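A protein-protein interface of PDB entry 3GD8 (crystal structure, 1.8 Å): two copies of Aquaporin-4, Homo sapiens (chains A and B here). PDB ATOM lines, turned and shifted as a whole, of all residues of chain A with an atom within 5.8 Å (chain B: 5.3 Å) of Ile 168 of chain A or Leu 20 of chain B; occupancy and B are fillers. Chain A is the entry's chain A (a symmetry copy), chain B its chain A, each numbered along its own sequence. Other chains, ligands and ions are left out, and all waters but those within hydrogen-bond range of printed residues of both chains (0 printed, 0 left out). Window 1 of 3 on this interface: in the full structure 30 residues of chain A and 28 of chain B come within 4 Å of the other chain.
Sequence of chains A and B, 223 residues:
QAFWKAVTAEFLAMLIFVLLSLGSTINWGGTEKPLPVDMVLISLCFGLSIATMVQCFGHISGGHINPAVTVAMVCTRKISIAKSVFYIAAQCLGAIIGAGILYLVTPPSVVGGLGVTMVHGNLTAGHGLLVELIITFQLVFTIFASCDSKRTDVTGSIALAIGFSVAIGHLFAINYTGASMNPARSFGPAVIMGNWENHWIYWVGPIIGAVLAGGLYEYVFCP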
ATOM      1  N   ILE A 134     -15.997 -21.689 -32.994  1.00  0.00           N
ATOM      2  CA  ILE A 134     -16.121 -22.653 -31.896  1.00  0.00           C
ATOM      3  C   ILE A 134     -15.447 -22.177 -30.602  1.00  0.00           C
ATOM      4  O   ILE A 134     -16.034 -22.288 -29.520  1.00  0.00           O
ATOM      5  CB  ILE A 134     -15.615 -24.027 -32.303  1.00  0.00           C
ATOM      6  CG1 ILE A 134     -16.494 -24.564 -33.436  1.00  0.00           C
ATOM      7  CG2 ILE A 134     -15.672 -25.004 -31.105  1.00  0.00           C
ATOM      8  CD1 ILE A 134     -16.026 -25.891 -34.040  1.00  0.00           C
ATOM      9  N   ILE A 135     -14.227 -21.661 -30.696  1.00  0.00           N
ATOM     10  CA  ILE A 135     -13.556 -21.193 -29.490  1.00  0.00           C
ATOM     11  C   ILE A 135     -14.277 -20.008 -28.854  1.00  0.00           C
ATOM     12  O   ILE A 135     -14.310 -19.906 -27.644  1.00  0.00           O
ATOM     13  CB  ILE A 135     -12.048 -20.920 -29.661  1.00  0.00           C
ATOM     14  CG1 ILE A 135     -11.754 -19.795 -30.666  1.00  0.00           C
ATOM     15  CG2 ILE A 135     -11.313 -22.226 -30.015  1.00  0.00           C
ATOM     16  CD1 ILE A 135     -10.236 -19.479 -30.766  1.00  0.00           C
ATOM     17  N   GLN A 138     -17.574 -21.341 -26.978  1.00  0.00           N
ATOM     18  CA  GLN A 138     -17.383 -21.918 -25.642  1.00  0.00           C
ATOM     19  C   GLN A 138     -17.098 -20.821 -24.612  1.00  0.00           C
ATOM     20  O   GLN A 138     -17.550 -20.896 -23.472  1.00  0.00           O
ATOM     21  CB  GLN A 138     -16.333 -23.044 -25.642  1.00  0.00           C
ATOM     22  CG  GLN A 138     -14.899 -22.676 -26.036  1.00  0.00           C
ATOM     23  CD  GLN A 138     -14.109 -22.082 -24.893  1.00  0.00           C
ATOM     24  OE1 GLN A 138     -14.357 -22.389 -23.721  1.00  0.00           O
ATOM     25  NE2 GLN A 138     -13.152 -21.219 -25.220  1.00  0.00           N
ATOM     26  N   GLY A 163     -11.523 -16.553 -17.576  1.00  0.00           N
ATOM     27  CA  GLY A 163     -10.124 -16.533 -17.977  1.00  0.00           C
ATOM     28  C   GLY A 163      -9.607 -17.887 -18.433  1.00  0.00           C
ATOM     29  O   GLY A 163      -8.873 -17.993 -19.422  1.00  0.00           O
ATOM     30  N   PHE A 164     -10.008 -18.952 -17.745  1.00  0.00           N
ATOM     31  CA  PHE A 164      -9.573 -20.279 -18.176  1.00  0.00           C
ATOM     32  C   PHE A 164     -10.234 -20.727 -19.487  1.00  0.00           C
ATOM     33  O   PHE A 164      -9.626 -21.478 -20.253  1.00  0.00           O
ATOM     34  CB  PHE A 164      -9.707 -21.323 -17.062  1.00  0.00           C
ATOM     35  CG  PHE A 164      -8.686 -21.160 -15.942  1.00  0.00           C
ATOM     36  CD1 PHE A 164      -7.366 -20.820 -16.206  1.00  0.00           C
ATOM     37  CD2 PHE A 164      -9.054 -21.382 -14.628  1.00  0.00           C
ATOM     38  CE1 PHE A 164      -6.424 -20.692 -15.168  1.00  0.00           C
ATOM     39  CE2 PHE A 164      -8.115 -21.267 -13.591  1.00  0.00           C
ATOM     40  CZ  PHE A 164      -6.816 -20.913 -13.866  1.00  0.00           C
ATOM     41  N   SER A 165     -11.448 -20.246 -19.763  1.00  0.00           N
ATOM     42  CA  SER A 165     -12.085 -20.465 -21.062  1.00  0.00           C
ATOM     43  C   SER A 165     -11.275 -19.798 -22.184  1.00  0.00           C
ATOM     44  O   SER A 165     -11.090 -20.371 -23.253  1.00  0.00           O
ATOM     45  CB  SER A 165     -13.522 -19.929 -21.069  1.00  0.00           C
ATOM     46  OG  SER A 165     -14.124 -20.164 -22.322  1.00  0.00           O
ATOM     47  N   VAL A 166     -10.791 -18.596 -21.919  1.00  0.00           N
ATOM     48  CA  VAL A 166      -9.880 -17.916 -22.845  1.00  0.00           C
ATOM     49  C   VAL A 166      -8.613 -18.749 -23.018  1.00  0.00           C
ATOM     50  O   VAL A 166      -8.146 -18.950 -24.144  1.00  0.00           O
ATOM     51  CB  VAL A 166      -9.582 -16.477 -22.388  1.00  0.00           C
ATOM     52  CG1 VAL A 166      -8.446 -15.816 -23.230  1.00  0.00           C
ATOM     53  CG2 VAL A 166     -10.862 -15.629 -22.466  1.00  0.00           C
ATOM     54  N   ALA A 167      -8.061 -19.239 -21.908  1.00  0.00           N
ATOM     55  CA  ALA A 167      -6.818 -20.013 -21.952  1.00  0.00           C
ATOM     56  C   ALA A 167      -6.951 -21.255 -22.845  1.00  0.00           C
ATOM     57  O   ALA A 167      -6.068 -21.519 -23.681  1.00  0.00           O
ATOM     58  CB  ALA A 167      -6.362 -20.386 -20.557  1.00  0.00           C
ATOM     59  N   ILE A 168      -8.039 -22.009 -22.697  1.00  0.00           N
ATOM     60  CA  ILE A 168      -8.214 -23.215 -23.514  1.00  0.00           C
ATOM     61  C   ILE A 168      -8.410 -22.928 -25.003  1.00  0.00           C
ATOM     62  O   ILE A 168      -7.961 -23.704 -25.856  1.00  0.00           O
ATOM     63  CB  ILE A 168      -9.312 -24.179 -22.975  1.00  0.00           C
ATOM     64  CG1 ILE A 168     -10.716 -23.581 -23.069  1.00  0.00           C
ATOM     65  CG2 ILE A 168      -8.980 -24.600 -21.529  1.00  0.00           C
ATOM     66  CD1 ILE A 168     -11.821 -24.550 -22.555  1.00  0.00           C
ATOM     67  N   GLY A 169      -9.050 -21.808 -25.313  1.00  0.00           N
ATOM     68  CA  GLY A 169      -9.164 -21.340 -26.687  1.00  0.00           C
ATOM     69  C   GLY A 169      -7.793 -21.178 -27.320  1.00  0.00           C
ATOM     70  O   GLY A 169      -7.588 -21.555 -28.477  1.00  0.00           O
ATOM     71  N   HIS A 170      -6.857 -20.638 -26.547  1.00  0.00           N
ATOM     72  CA  HIS A 170      -5.463 -20.484 -26.977  1.00  0.00           C
ATOM     73  C   HIS A 170      -4.680 -21.800 -27.047  1.00  0.00           C
ATOM     74  O   HIS A 170      -3.935 -22.060 -28.018  1.00  0.00           O
ATOM     75  CB  HIS A 170      -4.749 -19.498 -26.037  1.00  0.00           C
ATOM     76  CG  HIS A 170      -5.085 -18.069 -26.319  1.00  0.00           C
ATOM     77  ND1 HIS A 170      -6.275 -17.495 -25.928  1.00  0.00           N
ATOM     78  CD2 HIS A 170      -4.397 -17.104 -26.976  1.00  0.00           C
ATOM     79  CE1 HIS A 170      -6.308 -16.240 -26.344  1.00  0.00           C
ATOM     80  NE2 HIS A 170      -5.182 -15.982 -26.986  1.00  0.00           N
ATOM     81  N   LEU A 171      -4.820 -22.633 -26.018  1.00  0.00           N
ATOM     82  CA  LEU A 171      -4.058 -23.876 -25.963  1.00  0.00           C
ATOM     83  C   LEU A 171      -4.388 -24.765 -27.166  1.00  0.00           C
ATOM     84  O   LEU A 171      -3.536 -25.512 -27.636  1.00  0.00           O
ATOM     85  CB  LEU A 171      -4.315 -24.617 -24.645  1.00  0.00           C
ATOM     86  CG  LEU A 171      -3.783 -23.932 -23.384  1.00  0.00           C
ATOM     87  CD1 LEU A 171      -4.436 -24.500 -22.079  1.00  0.00           C
ATOM     88  CD2 LEU A 171      -2.239 -24.043 -23.319  1.00  0.00           C
ATOM     89  N   PHE A 172      -5.618 -24.660 -27.654  1.00  0.00           N
ATOM     90  CA  PHE A 172      -6.045 -25.295 -28.900  1.00  0.00           C
ATOM     91  C   PHE A 172      -5.597 -24.491 -30.134  1.00  0.00           C
ATOM     92  O   PHE A 172      -4.844 -24.995 -30.990  1.00  0.00           O
ATOM     93  CB  PHE A 172      -7.581 -25.441 -28.902  1.00  0.00           C
ATOM     94  CG  PHE A 172      -8.179 -25.790 -30.255  1.00  0.00           C
ATOM     95  CD1 PHE A 172      -7.546 -26.673 -31.114  1.00  0.00           C
ATOM     96  CD2 PHE A 172      -9.395 -25.236 -30.651  1.00  0.00           C
ATOM     97  CE1 PHE A 172      -8.104 -26.985 -32.374  1.00  0.00           C
ATOM     98  CE2 PHE A 172      -9.968 -25.544 -31.890  1.00  0.00           C
ATOM     99  CZ  PHE A 172      -9.333 -26.420 -32.747  1.00  0.00           C
ATOM    100  N   ALA A 173      -6.058 -23.250 -30.225  1.00  0.00           N
ATOM    101  CA  ALA A 173      -6.095 -22.547 -31.509  1.00  0.00           C
ATOM    102  C   ALA A 173      -4.956 -21.591 -31.849  1.00  0.00           C
ATOM    103  O   ALA A 173      -4.960 -21.049 -32.960  1.00  0.00           O
ATOM    104  CB  ALA A 173      -7.475 -21.822 -31.681  1.00  0.00           C
ATOM    105  N   MET A 181     -10.747 -14.933 -30.602  1.00  0.00           N
ATOM    106  CA  MET A 181     -11.969 -14.924 -29.788  1.00  0.00           C
ATOM    107  C   MET A 181     -12.529 -13.517 -29.533  1.00  0.00           C
ATOM    108  O   MET A 181     -13.458 -13.364 -28.735  1.00  0.00           O
ATOM    109  CB  MET A 181     -11.717 -15.606 -28.427  1.00  0.00           C
ATOM    110  CG  MET A 181     -10.809 -16.840 -28.470  1.00  0.00           C
ATOM    111  SD  MET A 181     -10.189 -17.322 -26.846  1.00  0.00           S
ATOM    112  CE  MET A 181     -11.529 -18.366 -26.300  1.00  0.00           C
ATOM    113  N   LEU B  15     -18.246 -32.704 -27.411  1.00  0.00           N
ATOM    114  CA  LEU B  15     -17.758 -32.199 -28.688  1.00  0.00           C
ATOM    115  C   LEU B  15     -16.697 -31.115 -28.462  1.00  0.00           C
ATOM    116  O   LEU B  15     -15.591 -31.181 -28.999  1.00  0.00           O
ATOM    117  CB  LEU B  15     -18.928 -31.671 -29.515  1.00  0.00           C
ATOM    118  CG  LEU B  15     -18.692 -31.182 -30.943  1.00  0.00           C
ATOM    119  CD1 LEU B  15     -20.039 -31.056 -31.686  1.00  0.00           C
ATOM    120  CD2 LEU B  15     -17.967 -29.858 -30.962  1.00  0.00           C
ATOM    121  N   ILE B  16     -17.027 -30.135 -27.637  1.00  0.00           N
ATOM    122  CA  ILE B  16     -16.115 -29.016 -27.391  1.00  0.00           C
ATOM    123  C   ILE B  16     -14.853 -29.460 -26.644  1.00  0.00           C
ATOM    124  O   ILE B  16     -13.727 -29.108 -27.036  1.00  0.00           O
ATOM    125  CB  ILE B  16     -16.823 -27.881 -26.622  1.00  0.00           C
ATOM    126  CG1 ILE B  16     -17.934 -27.285 -27.481  1.00  0.00           C
ATOM    127  CG2 ILE B  16     -15.815 -26.773 -26.209  1.00  0.00           C
ATOM    128  CD1 ILE B  16     -18.901 -26.410 -26.703  1.00  0.00           C
ATOM    129  N   PHE B  17     -15.044 -30.228 -25.574  1.00  0.00           N
ATOM    130  CA  PHE B  17     -13.936 -30.774 -24.804  1.00  0.00           C
ATOM    131  C   PHE B  17     -12.948 -31.512 -25.714  1.00  0.00           C
ATOM    132  O   PHE B  17     -11.746 -31.259 -25.674  1.00  0.00           O
ATOM    133  CB  PHE B  17     -14.486 -31.715 -23.729  1.00  0.00           C
ATOM    134  CG  PHE B  17     -13.466 -32.656 -23.149  1.00  0.00           C
ATOM    135  CD1 PHE B  17     -12.316 -32.173 -22.549  1.00  0.00           C
ATOM    136  CD2 PHE B  17     -13.680 -34.029 -23.175  1.00  0.00           C
ATOM    137  CE1 PHE B  17     -11.389 -33.042 -21.993  1.00  0.00           C
ATOM    138  CE2 PHE B  17     -12.749 -34.909 -22.628  1.00  0.00           C
ATOM    139  CZ  PHE B  17     -11.604 -34.412 -22.040  1.00  0.00           C
ATOM    140  N   VAL B  18     -13.467 -32.421 -26.531  1.00  0.00           N
ATOM    141  CA  VAL B  18     -12.618 -33.272 -27.376  1.00  0.00           C
ATOM    142  C   VAL B  18     -11.925 -32.463 -28.479  1.00  0.00           C
ATOM    143  O   VAL B  18     -10.721 -32.629 -28.703  1.00  0.00           O
ATOM    144  CB  VAL B  18     -13.430 -34.452 -27.948  1.00  0.00           C
ATOM    145  CG1 VAL B  18     -12.668 -35.201 -29.064  1.00  0.00           C
ATOM    146  CG2 VAL B  18     -13.856 -35.404 -26.804  1.00  0.00           C
ATOM    147  N   LEU B  19     -12.653 -31.565 -29.128  1.00  0.00           N
ATOM    148  CA  LEU B  19     -12.062 -30.741 -30.184  1.00  0.00           C
ATOM    149  C   LEU B  19     -10.874 -29.942 -29.646  1.00  0.00           C
ATOM    150  O   LEU B  19      -9.759 -30.018 -30.177  1.00  0.00           O
ATOM    151  CB  LEU B  19     -13.106 -29.827 -30.832  1.00  0.00           C
ATOM    152  CG  LEU B  19     -12.564 -28.795 -31.840  1.00  0.00           C
ATOM    153  CD1 LEU B  19     -11.831 -29.443 -33.010  1.00  0.00           C
ATOM    154  CD2 LEU B  19     -13.698 -27.908 -32.317  1.00  0.00           C
ATOM    155  N   LEU B  20     -11.103 -29.201 -28.573  1.00  0.00           N
ATOM    156  CA  LEU B  20     -10.062 -28.339 -28.018  1.00  0.00           C
ATOM    157  C   LEU B  20      -8.896 -29.145 -27.467  1.00  0.00           C
ATOM    158  O   LEU B  20      -7.729 -28.831 -27.722  1.00  0.00           O
ATOM    159  CB  LEU B  20     -10.632 -27.437 -26.922  1.00  0.00           C
ATOM    160  CG  LEU B  20     -11.172 -26.083 -27.400  1.00  0.00           C
ATOM    161  CD1 LEU B  20     -12.233 -26.237 -28.505  1.00  0.00           C
ATOM    162  CD2 LEU B  20     -11.714 -25.295 -26.212  1.00  0.00           C
ATOM    163  N   SER B  21      -9.203 -30.182 -26.708  1.00  0.00           N
ATOM    164  CA  SER B  21      -8.166 -30.923 -26.013  1.00  0.00           C
ATOM    165  C   SER B  21      -7.362 -31.808 -26.939  1.00  0.00           C
ATOM    166  O   SER B  21      -6.135 -31.822 -26.853  1.00  0.00           O
ATOM    167  CB  SER B  21      -8.759 -31.733 -24.870  1.00  0.00           C
ATOM    168  OG  SER B  21      -9.382 -30.847 -23.963  1.00  0.00           O
ATOM    169  N   LEU B  22      -8.020 -32.528 -27.845  1.00  0.00           N
ATOM    170  CA  LEU B  22      -7.250 -33.251 -28.858  1.00  0.00           C
ATOM    171  C   LEU B  22      -6.466 -32.263 -29.702  1.00  0.00           C
ATOM    172  O   LEU B  22      -5.336 -32.534 -30.123  1.00  0.00           O
ATOM    173  CB  LEU B  22      -8.147 -34.102 -29.757  1.00  0.00           C
ATOM    174  CG  LEU B  22      -8.892 -35.272 -29.127  1.00  0.00           C
ATOM    175  CD1 LEU B  22      -9.604 -36.080 -30.239  1.00  0.00           C
ATOM    176  CD2 LEU B  22      -7.986 -36.161 -28.332  1.00  0.00           C
ATOM    177  N   GLY B  23      -7.059 -31.099 -29.952  1.00  0.00           N
ATOM    178  CA  GLY B  23      -6.378 -30.059 -30.711  1.00  0.00           C
ATOM    179  C   GLY B  23      -5.064 -29.635 -30.070  1.00  0.00           C
ATOM    180  O   GLY B  23      -4.088 -29.386 -30.773  1.00  0.00           O
ATOM    181  N   SER B  24      -5.023 -29.602 -28.734  1.00  0.00           N
ATOM    182  CA  SER B  24      -3.809 -29.251 -28.007  1.00  0.00           C
ATOM    183  C   SER B  24      -2.684 -30.282 -28.191  1.00  0.00           C
ATOM    184  O   SER B  24      -1.516 -29.967 -27.948  1.00  0.00           O
ATOM    185  CB  SER B  24      -4.094 -29.040 -26.511  1.00  0.00           C
ATOM    186  OG  SER B  24      -4.174 -30.280 -25.842  1.00  0.00           O
ATOM    187  N   LEU B  44      -2.814 -29.044 -19.076  1.00  0.00           N
ATOM    188  CA  LEU B  44      -3.646 -27.867 -18.789  1.00  0.00           C
ATOM    189  C   LEU B  44      -4.857 -27.763 -19.700  1.00  0.00           C
ATOM    190  O   LEU B  44      -5.947 -27.396 -19.238  1.00  0.00           O
ATOM    191  CB  LEU B  44      -2.833 -26.575 -18.857  1.00  0.00           C
ATOM    192  CG  LEU B  44      -1.852 -26.373 -17.696  1.00  0.00           C
ATOM    193  CD1 LEU B  44      -1.126 -25.044 -17.853  1.00  0.00           C
ATOM    194  CD2 LEU B  44      -2.538 -26.429 -16.337  1.00  0.00           C
ATOM    195  N   CYS B  45      -4.701 -28.059 -20.988  1.00  0.00           N
ATOM    196  CA  CYS B  45      -5.844 -27.952 -21.868  1.00  0.00           C
ATOM    197  C   CYS B  45      -6.915 -28.973 -21.487  1.00  0.00           C
ATOM    198  O   CYS B  45      -8.084 -28.624 -21.409  1.00  0.00           O
ATOM    199  CB  CYS B  45      -5.462 -28.097 -23.341  1.00  0.00           C
ATOM    200  SG  CYS B  45      -6.805 -27.591 -24.440  1.00  0.00           S
ATOM    201  N   LEU B  48      -8.330 -27.875 -17.876  1.00  0.00           N
ATOM    202  CA  LEU B  48      -9.103 -26.628 -17.915  1.00  0.00           C
ATOM    203  C   LEU B  48     -10.315 -26.741 -18.825  1.00  0.00           C
ATOM    204  O   LEU B  48     -11.313 -26.052 -18.612  1.00  0.00           O
ATOM    205  CB  LEU B  48      -8.223 -25.461 -18.321  1.00  0.00           C
ATOM    206  CG  LEU B  48      -7.119 -25.122 -17.314  1.00  0.00           C
ATOM    207  CD1 LEU B  48      -6.253 -23.968 -17.870  1.00  0.00           C
ATOM    208  CD2 LEU B  48      -7.696 -24.781 -15.916  1.00  0.00           C
ATOM    209  N   SER B  49     -10.233 -27.595 -19.843  1.00  0.00           N
ATOM    210  CA  SER B  49     -11.386 -27.821 -20.707  1.00  0.00           C
ATOM    211  C   SER B  49     -12.516 -28.530 -19.960  1.00  0.00           C
ATOM    212  O   SER B  49     -13.684 -28.174 -20.121  1.00  0.00           O
ATOM    213  CB  SER B  49     -11.000 -28.587 -21.983  1.00  0.00           C
ATOM    214  OG  SER B  49     -10.254 -27.751 -22.856  1.00  0.00           O
ATOM    215  N   THR B  52     -14.023 -26.024 -17.608  1.00  0.00           N
ATOM    216  CA  THR B  52     -14.868 -25.098 -18.349  1.00  0.00           C
ATOM    217  C   THR B  52     -16.197 -25.753 -18.724  1.00  0.00           C
ATOM    218  O   THR B  52     -17.250 -25.136 -18.556  1.00  0.00           O
ATOM    219  CB  THR B  52     -14.103 -24.544 -19.586  1.00  0.00           C
ATOM    220  OG1 THR B  52     -12.922 -23.882 -19.132  1.00  0.00           O
ATOM    221  CG2 THR B  52     -14.946 -23.553 -20.391  1.00  0.00           C
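The backbone carbonyl oxygen (O) of Leu 20 of chain B sits at hydrogen-bond distance from the side-chain sulfur (SG) of Cys 45 of chain B (3.6 Å). O of Ser 21 of chain B is in hydrogen-bond range of OG of Ser 24 of chain B. The side-chain hydroxyl (OG) of Ser 49 of chain B is in hydrogen-bond range of the side-chain hydroxyl (OG) of Ser 21 of chain B (3.4 Å). The backbone carbonyl oxygen (O) of Leu 48 of chain B is in hydrogen-bond range of the side-chain hydroxyl (OG1) of Thr 52 of chain B (2.8 Å). The side-chain amide nitrogen of Gln 138 of chain A lies within hydrogen-bond range of the backbone carbonyl oxygen of Ile 135 of chain A (3.0 Å). The side-chain hydroxyl (OG) of Ser 165 of chain A lies within hydrogen-bond range of the side-chain amide oxygen (OE1) of Gln 138 of chain A, 2.6 Å away.
Among the printed residues, merely in contact across the chains: Ile 134 of chain A with Leu 19 of chain B, Gln 138 of chain A with Ile 16 of chain B, Gln 138 of chain A with Thr 52 of chain B, Phe 164 of chain A with Leu 48 of chain B, Ser 165 of chain A with Thr 52 of chain B, Ile 168 of chain A with Leu 20 of chain B, Ile 168 of chain A with Leu 48 of chain B, Ile 168 of chain A with Ser 49 of chain B, Ile 168 of chain A with Thr 52 of chain B, Leu 171 of chain A with Ser 24 of chain B, Leu 171 of chain A with Cys 45 of chain B, Phe 172 of chain A with Leu 19 of chain B, Phe 172 of chain A with Leu 20 of chain B and Phe 172 of chain A with Gly 23 of chain B.
Gly 163 of chain A touches none of the printed residues of chain B. Printed residues of chain B within 4 Å of Ser 165 of chain A: Thr 52 (3.95 Å). Ile 168 of chain A touches four residues of chain B. Of the printed residues of chain A, Leu 20 of chain B touches Ile 168 (3.7 Å) and Phe 172 (3.6 Å). Of the printed residues of chain A, Gly 23 of chain B touches Phe 172. Of the printed residues of chain A, Leu 48 of chain B touches Phe 164 (3.7 Å) and Ile 168 (3.4 Å). Printed residues of chain A within 4 Å of Ser 49 of chain B: Ile 168. The nearest printed residue of chain A that does not touch Leu 48 of chain B is Ala 167 of chain A (4.5 Å).
Of the 15 printed residues of chain B, 9 touch a printed residue of chain A. Hydrophobic or aromatic side chains of chain B within 4 Å of the printed part of chain A: Ile 16, Leu 19, Leu 20 and Leu 48. Along chain B the printed residues that touch a printed residue of chain A span positions 16 to 52. Of the 15 printed residues of chain A, 7 touch a printed residue of chain B. Printed residues of chain A that touch a printed residue of chain B: Ile 134, Gln 138, Phe 164, Ser 165, Ile 168, Leu 171 and Phe 172. Among the printed residues, 14 pairs touch across the chains.
No position is printed for both chains. Of the 14 pairs that touch across the chains among the printed residues, none has its exchanged pair printed and touching as well.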
